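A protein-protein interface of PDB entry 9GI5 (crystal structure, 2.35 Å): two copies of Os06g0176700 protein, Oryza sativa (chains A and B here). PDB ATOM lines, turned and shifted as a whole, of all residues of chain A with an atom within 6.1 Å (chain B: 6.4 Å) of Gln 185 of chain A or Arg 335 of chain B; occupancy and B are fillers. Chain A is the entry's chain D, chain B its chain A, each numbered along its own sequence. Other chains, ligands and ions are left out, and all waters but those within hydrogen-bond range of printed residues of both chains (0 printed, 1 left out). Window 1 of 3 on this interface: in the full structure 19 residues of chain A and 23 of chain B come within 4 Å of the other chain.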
ATOM      1  N   ARG A 178     -17.388  22.427 -14.817  1.00  0.00           N
ATOM      2  CA  ARG A 178     -18.124  23.380 -15.638  1.00  0.00           C
ATOM      3  C   ARG A 178     -17.586  23.404 -17.064  1.00  0.00           C
ATOM      4  O   ARG A 178     -18.350  23.556 -18.026  1.00  0.00           O
ATOM      5  CB  ARG A 178     -18.058  24.770 -15.006  1.00  0.00           C
ATOM      6  CG  ARG A 178     -18.546  25.895 -15.907  1.00  0.00           C
ATOM      7  CD  ARG A 178     -17.491  26.976 -16.044  1.00  0.00           C
ATOM      8  NE  ARG A 178     -17.425  27.809 -14.850  1.00  0.00           N
ATOM      9  CZ  ARG A 178     -16.315  28.374 -14.398  1.00  0.00           C
ATOM     10  NH1 ARG A 178     -15.160  28.234 -15.029  1.00  0.00           N
ATOM     11  NH2 ARG A 178     -16.364  29.093 -13.279  1.00  0.00           N
ATOM     12  N   ARG A 180     -16.129  20.800 -18.572  1.00  0.00           N
ATOM     13  CA  ARG A 180     -16.647  19.569 -19.159  1.00  0.00           C
ATOM     14  C   ARG A 180     -18.076  19.754 -19.653  1.00  0.00           C
ATOM     15  O   ARG A 180     -18.413  19.365 -20.779  1.00  0.00           O
ATOM     16  CB  ARG A 180     -16.578  18.430 -18.139  1.00  0.00           C
ATOM     17  CG  ARG A 180     -17.127  17.102 -18.645  1.00  0.00           C
ATOM     18  CD  ARG A 180     -17.536  16.172 -17.499  1.00  0.00           C
ATOM     19  NE  ARG A 180     -18.936  16.324 -17.113  1.00  0.00           N
ATOM     20  CZ  ARG A 180     -19.365  16.429 -15.862  1.00  0.00           C
ATOM     21  NH1 ARG A 180     -18.524  16.426 -14.841  1.00  0.00           N
ATOM     22  NH2 ARG A 180     -20.672  16.528 -15.631  1.00  0.00           N
ATOM     23  N   ASP A 181     -18.929  20.367 -18.827  1.00  0.00           N
ATOM     24  CA  ASP A 181     -20.336  20.516 -19.186  1.00  0.00           C
ATOM     25  C   ASP A 181     -20.507  21.432 -20.395  1.00  0.00           C
ATOM     26  O   ASP A 181     -21.219  21.091 -21.347  1.00  0.00           O
ATOM     27  CB  ASP A 181     -21.135  21.038 -17.990  1.00  0.00           C
ATOM     28  CG  ASP A 181     -21.152  20.057 -16.826  1.00  0.00           C
ATOM     29  OD1 ASP A 181     -21.200  20.508 -15.658  1.00  0.00           O
ATOM     30  OD2 ASP A 181     -21.083  18.835 -17.075  1.00  0.00           O
ATOM     31  N   ASP A 182     -19.856  22.600 -20.379  1.00  0.00           N
ATOM     32  CA  ASP A 182     -20.031  23.561 -21.466  1.00  0.00           C
ATOM     33  C   ASP A 182     -19.593  22.978 -22.802  1.00  0.00           C
ATOM     34  O   ASP A 182     -20.320  23.062 -23.799  1.00  0.00           O
ATOM     35  CB  ASP A 182     -19.257  24.844 -21.164  1.00  0.00           C
ATOM     36  CG  ASP A 182     -19.905  25.674 -20.075  1.00  0.00           C
ATOM     37  OD1 ASP A 182     -21.002  25.305 -19.613  1.00  0.00           O
ATOM     38  OD2 ASP A 182     -19.303  26.685 -19.665  1.00  0.00           O
ATOM     39  N   ILE A 183     -18.409  22.367 -22.836  1.00  0.00           N
ATOM     40  CA  ILE A 183     -17.878  21.842 -24.091  1.00  0.00           C
ATOM     41  C   ILE A 183     -18.750  20.699 -24.604  1.00  0.00           C
ATOM     42  O   ILE A 183     -19.037  20.609 -25.806  1.00  0.00           O
ATOM     43  CB  ILE A 183     -16.410  21.416 -23.909  1.00  0.00           C
ATOM     44  CG1 ILE A 183     -15.469  22.596 -24.176  1.00  0.00           C
ATOM     45  CG2 ILE A 183     -16.059  20.266 -24.841  1.00  0.00           C
ATOM     46  CD1 ILE A 183     -15.556  23.712 -23.164  1.00  0.00           C
ATOM     47  N   VAL A 184     -19.200  19.820 -23.704  1.00  0.00           N
ATOM     48  CA  VAL A 184     -20.063  18.711 -24.105  1.00  0.00           C
ATOM     49  C   VAL A 184     -21.362  19.241 -24.705  1.00  0.00           C
ATOM     50  O   VAL A 184     -21.813  18.777 -25.761  1.00  0.00           O
ATOM     51  CB  VAL A 184     -20.325  17.780 -22.909  1.00  0.00           C
ATOM     52  CG1 VAL A 184     -21.649  17.052 -23.071  1.00  0.00           C
ATOM     53  CG2 VAL A 184     -19.186  16.778 -22.760  1.00  0.00           C
ATOM     54  N   GLN A 185     -21.974  20.234 -24.046  1.00  0.00           N
ATOM     55  CA  GLN A 185     -23.186  20.844 -24.586  1.00  0.00           C
ATOM     56  C   GLN A 185     -22.933  21.451 -25.959  1.00  0.00           C
ATOM     57  O   GLN A 185     -23.735  21.269 -26.881  1.00  0.00           O
ATOM     58  CB  GLN A 185     -23.722  21.910 -23.628  1.00  0.00           C
ATOM     59  CG  GLN A 185     -25.158  22.344 -23.929  1.00  0.00           C
ATOM     60  CD  GLN A 185     -25.530  23.664 -23.269  1.00  0.00           C
ATOM     61  OE1 GLN A 185     -24.664  24.396 -22.785  1.00  0.00           O
ATOM     62  NE2 GLN A 185     -26.823  23.969 -23.242  1.00  0.00           N
ATOM     63  N   ALA A 186     -21.814  22.165 -26.117  1.00  0.00           N
ATOM     64  CA  ALA A 186     -21.512  22.807 -27.393  1.00  0.00           C
ATOM     65  C   ALA A 186     -21.399  21.780 -28.510  1.00  0.00           C
ATOM     66  O   ALA A 186     -21.964  21.955 -29.596  1.00  0.00           O
ATOM     67  CB  ALA A 186     -20.222  23.617 -27.279  1.00  0.00           C
ATOM     68  N   MET A 187     -20.684  20.686 -28.250  1.00  0.00           N
ATOM     69  CA  MET A 187     -20.443  19.693 -29.290  1.00  0.00           C
ATOM     70  C   MET A 187     -21.712  18.931 -29.643  1.00  0.00           C
ATOM     71  O   MET A 187     -21.889  18.521 -30.796  1.00  0.00           O
ATOM     72  CB  MET A 187     -19.344  18.739 -28.832  1.00  0.00           C
ATOM     73  CG  MET A 187     -18.039  19.446 -28.493  1.00  0.00           C
ATOM     74  SD  MET A 187     -16.766  18.298 -27.937  1.00  0.00           S
ATOM     75  CE  MET A 187     -17.294  16.828 -28.784  1.00  0.00           C
ATOM     76  N   SER A 188     -22.604  18.736 -28.671  1.00  0.00           N
ATOM     77  CA  SER A 188     -23.873  18.079 -28.955  1.00  0.00           C
ATOM     78  C   SER A 188     -24.693  18.891 -29.947  1.00  0.00           C
ATOM     79  O   SER A 188     -25.300  18.330 -30.868  1.00  0.00           O
ATOM     80  CB  SER A 188     -24.653  17.857 -27.658  1.00  0.00           C
ATOM     81  OG  SER A 188     -23.984  16.931 -26.818  1.00  0.00           O
ATOM     82  N   LYS A 189     -24.724  20.214 -29.777  1.00  0.00           N
ATOM     83  CA  LYS A 189     -25.355  21.069 -30.779  1.00  0.00           C
ATOM     84  C   LYS A 189     -24.606  20.997 -32.103  1.00  0.00           C
ATOM     85  O   LYS A 189     -25.223  20.914 -33.173  1.00  0.00           O
ATOM     86  CB  LYS A 189     -25.430  22.511 -30.272  1.00  0.00           C
ATOM     87  CG  LYS A 189     -26.329  22.684 -29.059  1.00  0.00           C
ATOM     88  CD  LYS A 189     -26.919  24.091 -28.955  1.00  0.00           C
ATOM     89  CE  LYS A 189     -25.939  25.091 -28.352  1.00  0.00           C
ATOM     90  NZ  LYS A 189     -25.888  26.350 -29.167  1.00  0.00           N
ATOM     91  N   LEU A 190     -23.271  21.008 -32.049  1.00  0.00           N
ATOM     92  CA  LEU A 190     -22.484  20.901 -33.273  1.00  0.00           C
ATOM     93  C   LEU A 190     -22.781  19.608 -34.018  1.00  0.00           C
ATOM     94  O   LEU A 190     -22.729  19.575 -35.252  1.00  0.00           O
ATOM     95  CB  LEU A 190     -20.993  20.990 -32.953  1.00  0.00           C
ATOM     96  CG  LEU A 190     -20.443  22.371 -32.603  1.00  0.00           C
ATOM     97  CD1 LEU A 190     -18.941  22.296 -32.410  1.00  0.00           C
ATOM     98  CD2 LEU A 190     -20.800  23.381 -33.680  1.00  0.00           C
ATOM     99  N   GLU A 195     -28.886  18.495 -26.771  1.00  0.00           N
ATOM    100  CA  GLU A 195     -27.728  19.043 -26.071  1.00  0.00           C
ATOM    101  C   GLU A 195     -27.500  18.410 -24.707  1.00  0.00           C
ATOM    102  O   GLU A 195     -26.461  18.677 -24.096  1.00  0.00           O
ATOM    103  CB  GLU A 195     -27.805  20.568 -25.931  1.00  0.00           C
ATOM    104  CG  GLU A 195     -29.139  21.182 -25.561  1.00  0.00           C
ATOM    105  CD  GLU A 195     -29.194  22.651 -25.977  1.00  0.00           C
ATOM    106  OE1 GLU A 195     -28.442  23.458 -25.383  1.00  0.00           O
ATOM    107  OE2 GLU A 195     -29.934  22.985 -26.932  1.00  0.00           O
ATOM    108  N   ASP A 196     -28.419  17.584 -24.218  1.00  0.00           N
ATOM    109  CA  ASP A 196     -28.175  16.787 -23.023  1.00  0.00           C
ATOM    110  C   ASP A 196     -27.837  15.335 -23.349  1.00  0.00           C
ATOM    111  O   ASP A 196     -27.837  14.496 -22.443  1.00  0.00           O
ATOM    112  CB  ASP A 196     -29.382  16.846 -22.078  1.00  0.00           C
ATOM    113  CG  ASP A 196     -30.671  16.387 -22.738  1.00  0.00           C
ATOM    114  OD1 ASP A 196     -30.786  16.467 -23.982  1.00  0.00           O
ATOM    115  OD2 ASP A 196     -31.582  15.954 -22.002  1.00  0.00           O
ATOM    116  N   PHE A 199     -25.018  13.436 -21.192  1.00  0.00           N
ATOM    117  CA  PHE A 199     -24.989  13.526 -19.738  1.00  0.00           C
ATOM    118  C   PHE A 199     -25.485  12.268 -19.047  1.00  0.00           C
ATOM    119  O   PHE A 199     -25.110  12.031 -17.893  1.00  0.00           O
ATOM    120  CB  PHE A 199     -25.802  14.734 -19.264  1.00  0.00           C
ATOM    121  CG  PHE A 199     -25.123  16.042 -19.531  1.00  0.00           C
ATOM    122  CD1 PHE A 199     -24.104  16.482 -18.710  1.00  0.00           C
ATOM    123  CD2 PHE A 199     -25.487  16.818 -20.621  1.00  0.00           C
ATOM    124  CE1 PHE A 199     -23.461  17.674 -18.958  1.00  0.00           C
ATOM    125  CE2 PHE A 199     -24.848  18.016 -20.874  1.00  0.00           C
ATOM    126  CZ  PHE A 199     -23.834  18.443 -20.043  1.00  0.00           C
ATOM    127  N   ILE B 311     -26.234  21.549  -8.203  1.00  0.00           N
ATOM    128  CA  ILE B 311     -27.597  21.862  -7.800  1.00  0.00           C
ATOM    129  C   ILE B 311     -28.188  20.639  -7.111  1.00  0.00           C
ATOM    130  O   ILE B 311     -28.184  19.536  -7.668  1.00  0.00           O
ATOM    131  CB  ILE B 311     -28.441  22.293  -9.010  1.00  0.00           C
ATOM    132  CG1 ILE B 311     -27.878  23.583  -9.615  1.00  0.00           C
ATOM    133  CG2 ILE B 311     -29.898  22.481  -8.615  1.00  0.00           C
ATOM    134  CD1 ILE B 311     -28.609  24.032 -10.861  1.00  0.00           C
ATOM    135  N   SER B 330     -24.665  18.849 -11.696  1.00  0.00           N
ATOM    136  CA  SER B 330     -23.905  20.056 -11.963  1.00  0.00           C
ATOM    137  C   SER B 330     -24.759  21.076 -12.707  1.00  0.00           C
ATOM    138  O   SER B 330     -25.768  20.748 -13.340  1.00  0.00           O
ATOM    139  CB  SER B 330     -22.660  19.737 -12.788  1.00  0.00           C
ATOM    140  OG  SER B 330     -23.017  19.440 -14.130  1.00  0.00           O
ATOM    141  N   VAL B 331     -24.330  22.334 -12.624  1.00  0.00           N
ATOM    142  CA  VAL B 331     -25.121  23.432 -13.167  1.00  0.00           C
ATOM    143  C   VAL B 331     -25.251  23.303 -14.679  1.00  0.00           C
ATOM    144  O   VAL B 331     -26.338  23.483 -15.241  1.00  0.00           O
ATOM    145  CB  VAL B 331     -24.495  24.775 -12.756  1.00  0.00           C
ATOM    146  CG1 VAL B 331     -25.047  25.903 -13.612  1.00  0.00           C
ATOM    147  CG2 VAL B 331     -24.751  25.012 -11.287  1.00  0.00           C
ATOM    148  N   GLY B 332     -24.146  22.984 -15.359  1.00  0.00           N
ATOM    149  CA  GLY B 332     -24.200  22.823 -16.801  1.00  0.00           C
ATOM    150  C   GLY B 332     -25.076  21.661 -17.223  1.00  0.00           C
ATOM    151  O   GLY B 332     -25.826  21.759 -18.196  1.00  0.00           O
ATOM    152  N   GLU B 333     -24.991  20.544 -16.494  1.00  0.00           N
ATOM    153  CA  GLU B 333     -25.859  19.407 -16.775  1.00  0.00           C
ATOM    154  C   GLU B 333     -27.322  19.782 -16.585  1.00  0.00           C
ATOM    155  O   GLU B 333     -28.171  19.450 -17.420  1.00  0.00           O
ATOM    156  CB  GLU B 333     -25.483  18.223 -15.881  1.00  0.00           C
ATOM    157  CG  GLU B 333     -26.452  17.057 -15.971  1.00  0.00           C
ATOM    158  CD  GLU B 333     -25.972  15.817 -15.226  1.00  0.00           C
ATOM    159  OE1 GLU B 333     -24.970  15.899 -14.476  1.00  0.00           O
ATOM    160  OE2 GLU B 333     -26.607  14.755 -15.392  1.00  0.00           O
ATOM    161  N   PHE B 334     -27.627  20.487 -15.493  1.00  0.00           N
ATOM    162  CA  PHE B 334     -28.977  20.987 -15.256  1.00  0.00           C
ATOM    163  C   PHE B 334     -29.454  21.846 -16.420  1.00  0.00           C
ATOM    164  O   PHE B 334     -30.559  21.655 -16.941  1.00  0.00           O
ATOM    165  CB  PHE B 334     -28.988  21.794 -13.956  1.00  0.00           C
ATOM    166  CG  PHE B 334     -30.360  22.074 -13.412  1.00  0.00           C
ATOM    167  CD1 PHE B 334     -31.091  23.160 -13.864  1.00  0.00           C
ATOM    168  CD2 PHE B 334     -30.898  21.278 -12.410  1.00  0.00           C
ATOM    169  CE1 PHE B 334     -32.353  23.428 -13.353  1.00  0.00           C
ATOM    170  CE2 PHE B 334     -32.158  21.542 -11.896  1.00  0.00           C
ATOM    171  CZ  PHE B 334     -32.884  22.619 -12.369  1.00  0.00           C
ATOM    172  N   ARG B 335     -28.618  22.801 -16.839  1.00  0.00           N
ATOM    173  CA  ARG B 335     -29.007  23.752 -17.873  1.00  0.00           C
ATOM    174  C   ARG B 335     -29.257  23.054 -19.205  1.00  0.00           C
ATOM    175  O   ARG B 335     -30.253  23.335 -19.884  1.00  0.00           O
ATOM    176  CB  ARG B 335     -27.921  24.825 -18.012  1.00  0.00           C
ATOM    177  CG  ARG B 335     -28.151  25.841 -19.117  1.00  0.00           C
ATOM    178  CD  ARG B 335     -26.867  26.111 -19.900  1.00  0.00           C
ATOM    179  NE  ARG B 335     -25.730  26.337 -19.019  1.00  0.00           N
ATOM    180  CZ  ARG B 335     -24.535  25.778 -19.163  1.00  0.00           C
ATOM    181  NH1 ARG B 335     -24.266  24.969 -20.173  1.00  0.00           N
ATOM    182  NH2 ARG B 335     -23.592  26.025 -18.257  1.00  0.00           N
ATOM    183  N   ALA B 336     -28.372  22.133 -19.593  1.00  0.00           N
ATOM    184  CA  ALA B 336     -28.551  21.438 -20.865  1.00  0.00           C
ATOM    185  C   ALA B 336     -29.757  20.510 -20.826  1.00  0.00           C
ATOM    186  O   ALA B 336     -30.421  20.307 -21.855  1.00  0.00           O
ATOM    187  CB  ALA B 336     -27.288  20.655 -21.222  1.00  0.00           C
ATOM    188  N   GLY B 337     -30.043  19.937 -19.653  1.00  0.00           N
ATOM    189  CA  GLY B 337     -31.237  19.126 -19.498  1.00  0.00           C
ATOM    190  C   GLY B 337     -32.512  19.941 -19.554  1.00  0.00           C
ATOM    191  O   GLY B 337     -33.508  19.503 -20.129  1.00  0.00           O
ATOM    192  N   ILE B 338     -32.511  21.124 -18.935  1.00  0.00           N
ATOM    193  CA  ILE B 338     -33.666  22.012 -19.038  1.00  0.00           C
ATOM    194  C   ILE B 338     -33.945  22.338 -20.502  1.00  0.00           C
ATOM    195  O   ILE B 338     -35.079  22.232 -20.981  1.00  0.00           O
ATOM    196  CB  ILE B 338     -33.434  23.298 -18.222  1.00  0.00           C
ATOM    197  CG1 ILE B 338     -33.465  23.024 -16.713  1.00  0.00           C
ATOM    198  CG2 ILE B 338     -34.453  24.369 -18.617  1.00  0.00           C
ATOM    199  CD1 ILE B 338     -34.851  22.813 -16.140  1.00  0.00           C
ATOM    200  N   ILE B 339     -32.903  22.745 -21.229  1.00  0.00           N
ATOM    201  CA  ILE B 339     -33.064  23.196 -22.607  1.00  0.00           C
ATOM    202  C   ILE B 339     -33.376  22.027 -23.534  1.00  0.00           C
ATOM    203  O   ILE B 339     -34.236  22.131 -24.417  1.00  0.00           O
ATOM    204  CB  ILE B 339     -31.803  23.961 -23.046  1.00  0.00           C
ATOM    205  CG1 ILE B 339     -31.607  25.194 -22.155  1.00  0.00           C
ATOM    206  CG2 ILE B 339     -31.889  24.344 -24.508  1.00  0.00           C
ATOM    207  CD1 ILE B 339     -30.377  26.009 -22.501  1.00  0.00           C
ATOM    208  N   GLY B 340     -32.680  20.903 -23.367  1.00  0.00           N
ATOM    209  CA  GLY B 340     -32.950  19.757 -24.220  1.00  0.00           C
ATOM    210  C   GLY B 340     -34.337  19.185 -23.995  1.00  0.00           C
ATOM    211  O   GLY B 340     -35.079  18.941 -24.950  1.00  0.00           O
ATOM    212  N   TYR B 348     -37.660  18.189 -17.254  1.00  0.00           N
ATOM    213  CA  TYR B 348     -36.351  17.740 -16.796  1.00  0.00           C
ATOM    214  C   TYR B 348     -36.367  17.358 -15.324  1.00  0.00           C
ATOM    215  O   TYR B 348     -35.742  16.367 -14.929  1.00  0.00           O
ATOM    216  CB  TYR B 348     -35.307  18.832 -17.036  1.00  0.00           C
ATOM    217  CG  TYR B 348     -33.941  18.512 -16.453  1.00  0.00           C
ATOM    218  CD1 TYR B 348     -33.230  17.395 -16.881  1.00  0.00           C
ATOM    219  CD2 TYR B 348     -33.368  19.320 -15.476  1.00  0.00           C
ATOM    220  CE1 TYR B 348     -31.990  17.094 -16.365  1.00  0.00           C
ATOM    221  CE2 TYR B 348     -32.117  19.025 -14.941  1.00  0.00           C
ATOM    222  CZ  TYR B 348     -31.431  17.907 -15.396  1.00  0.00           C
ATOM    223  OH  TYR B 348     -30.186  17.584 -14.893  1.00  0.00           O
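OG of Ser 330 of chain B sits at hydrogen-bond distance from OD1 of Asp 181 of chain A, 2.6 Å away. The guanidinium group of Arg 335 of chain B is in salt-bridge range of the side-chain carboxylate of Asp 182 of chain A (3.0 Å). The guanidinium group of Arg 335 of chain B is in hydrogen-bond range of the side-chain amide oxygen of Gln 185 of chain A, 2.7 Å away.
NH2 of Arg 180 of chain A lies within salt-bridge range of OD2 of Asp 181 of chain A, 2.8 Å away. OG of Ser 330 of chain B lies close to N of Glu 333 of chain B. NE2 of Gln 185 of chain A lies within hydrogen-bond range of OE1 of Glu 195 of chain A, at 2.7 Å.
Among the printed residues, merely in contact across the chains: Glu 195 of chain A with Ile 339 of chain B (3.4 Å), Glu 195 of chain A with Ala 336 of chain B (3.6 Å), Phe 199 of chain A with Glu 333 of chain B (3.6 Å), Phe 199 of chain A with Ala 336 of chain B (3.6 Å), Asp 196 of chain A with Ala 336 of chain B (3.6 Å), Asp 181 of chain A with Gly 332 of chain B (3.7 Å), Gln 185 of chain A with Ala 336 of chain B (3.8 Å), Asp 181 of chain A with Glu 333 of chain B (3.9 Å), Asp 196 of chain A with Gly 337 of chain B (3.9 Å) and Asp 196 of chain A with Gly 340 of chain B (3.9 Å).
Of the printed residues of chain B, Gln 185 of chain A touches Arg 335 (2.7 Å) and Ala 336 (3.8 Å). Ser 188 of chain A touches none of the printed residues of chain B. Of the printed residues of chain B, Glu 195 of chain A touches Ala 336 and Ile 339. Of chain A, only Asp 182 (3.0 Å) and Gln 185 (2.7 Å) come within 4 Å of Arg 335 of chain B. Of the printed residues of chain A, Ile 339 of chain B touches Glu 195 (3.4 Å). The nearest residue of chain A that does not touch Arg 335 of chain B is Asp 181 of chain A (5.1 Å).
Printed residues of chain A that touch a printed residue of chain B: Asp 181, Asp 182, Gln 185, Glu 195, Asp 196 and Phe 199. Hydrophobic or aromatic side chains of chain A within 4 Å of the printed part of chain B: Phe 199. Of the 13 printed residues of chain B, 8 touch a printed residue of chain A. Printed residues of chain B that touch a printed residue of chain A: Ser 330, Gly 332, Glu 333, Arg 335, Ala 336, Gly 337, Ile 339 and Gly 340. Among the printed residues, 13 pairs touch across the chains. Among the printed residues, Asp or Glu carboxylates within 4 Å of a Lys or Arg side-chain nitrogen of the other chain: Asp 182 of chain A with Arg 335 of chain B (3.0 Å).
No position is printed for both chains. Of the 13 pairs that touch across the chains among the printed residues, none has its exchanged pair printed and touching as well.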
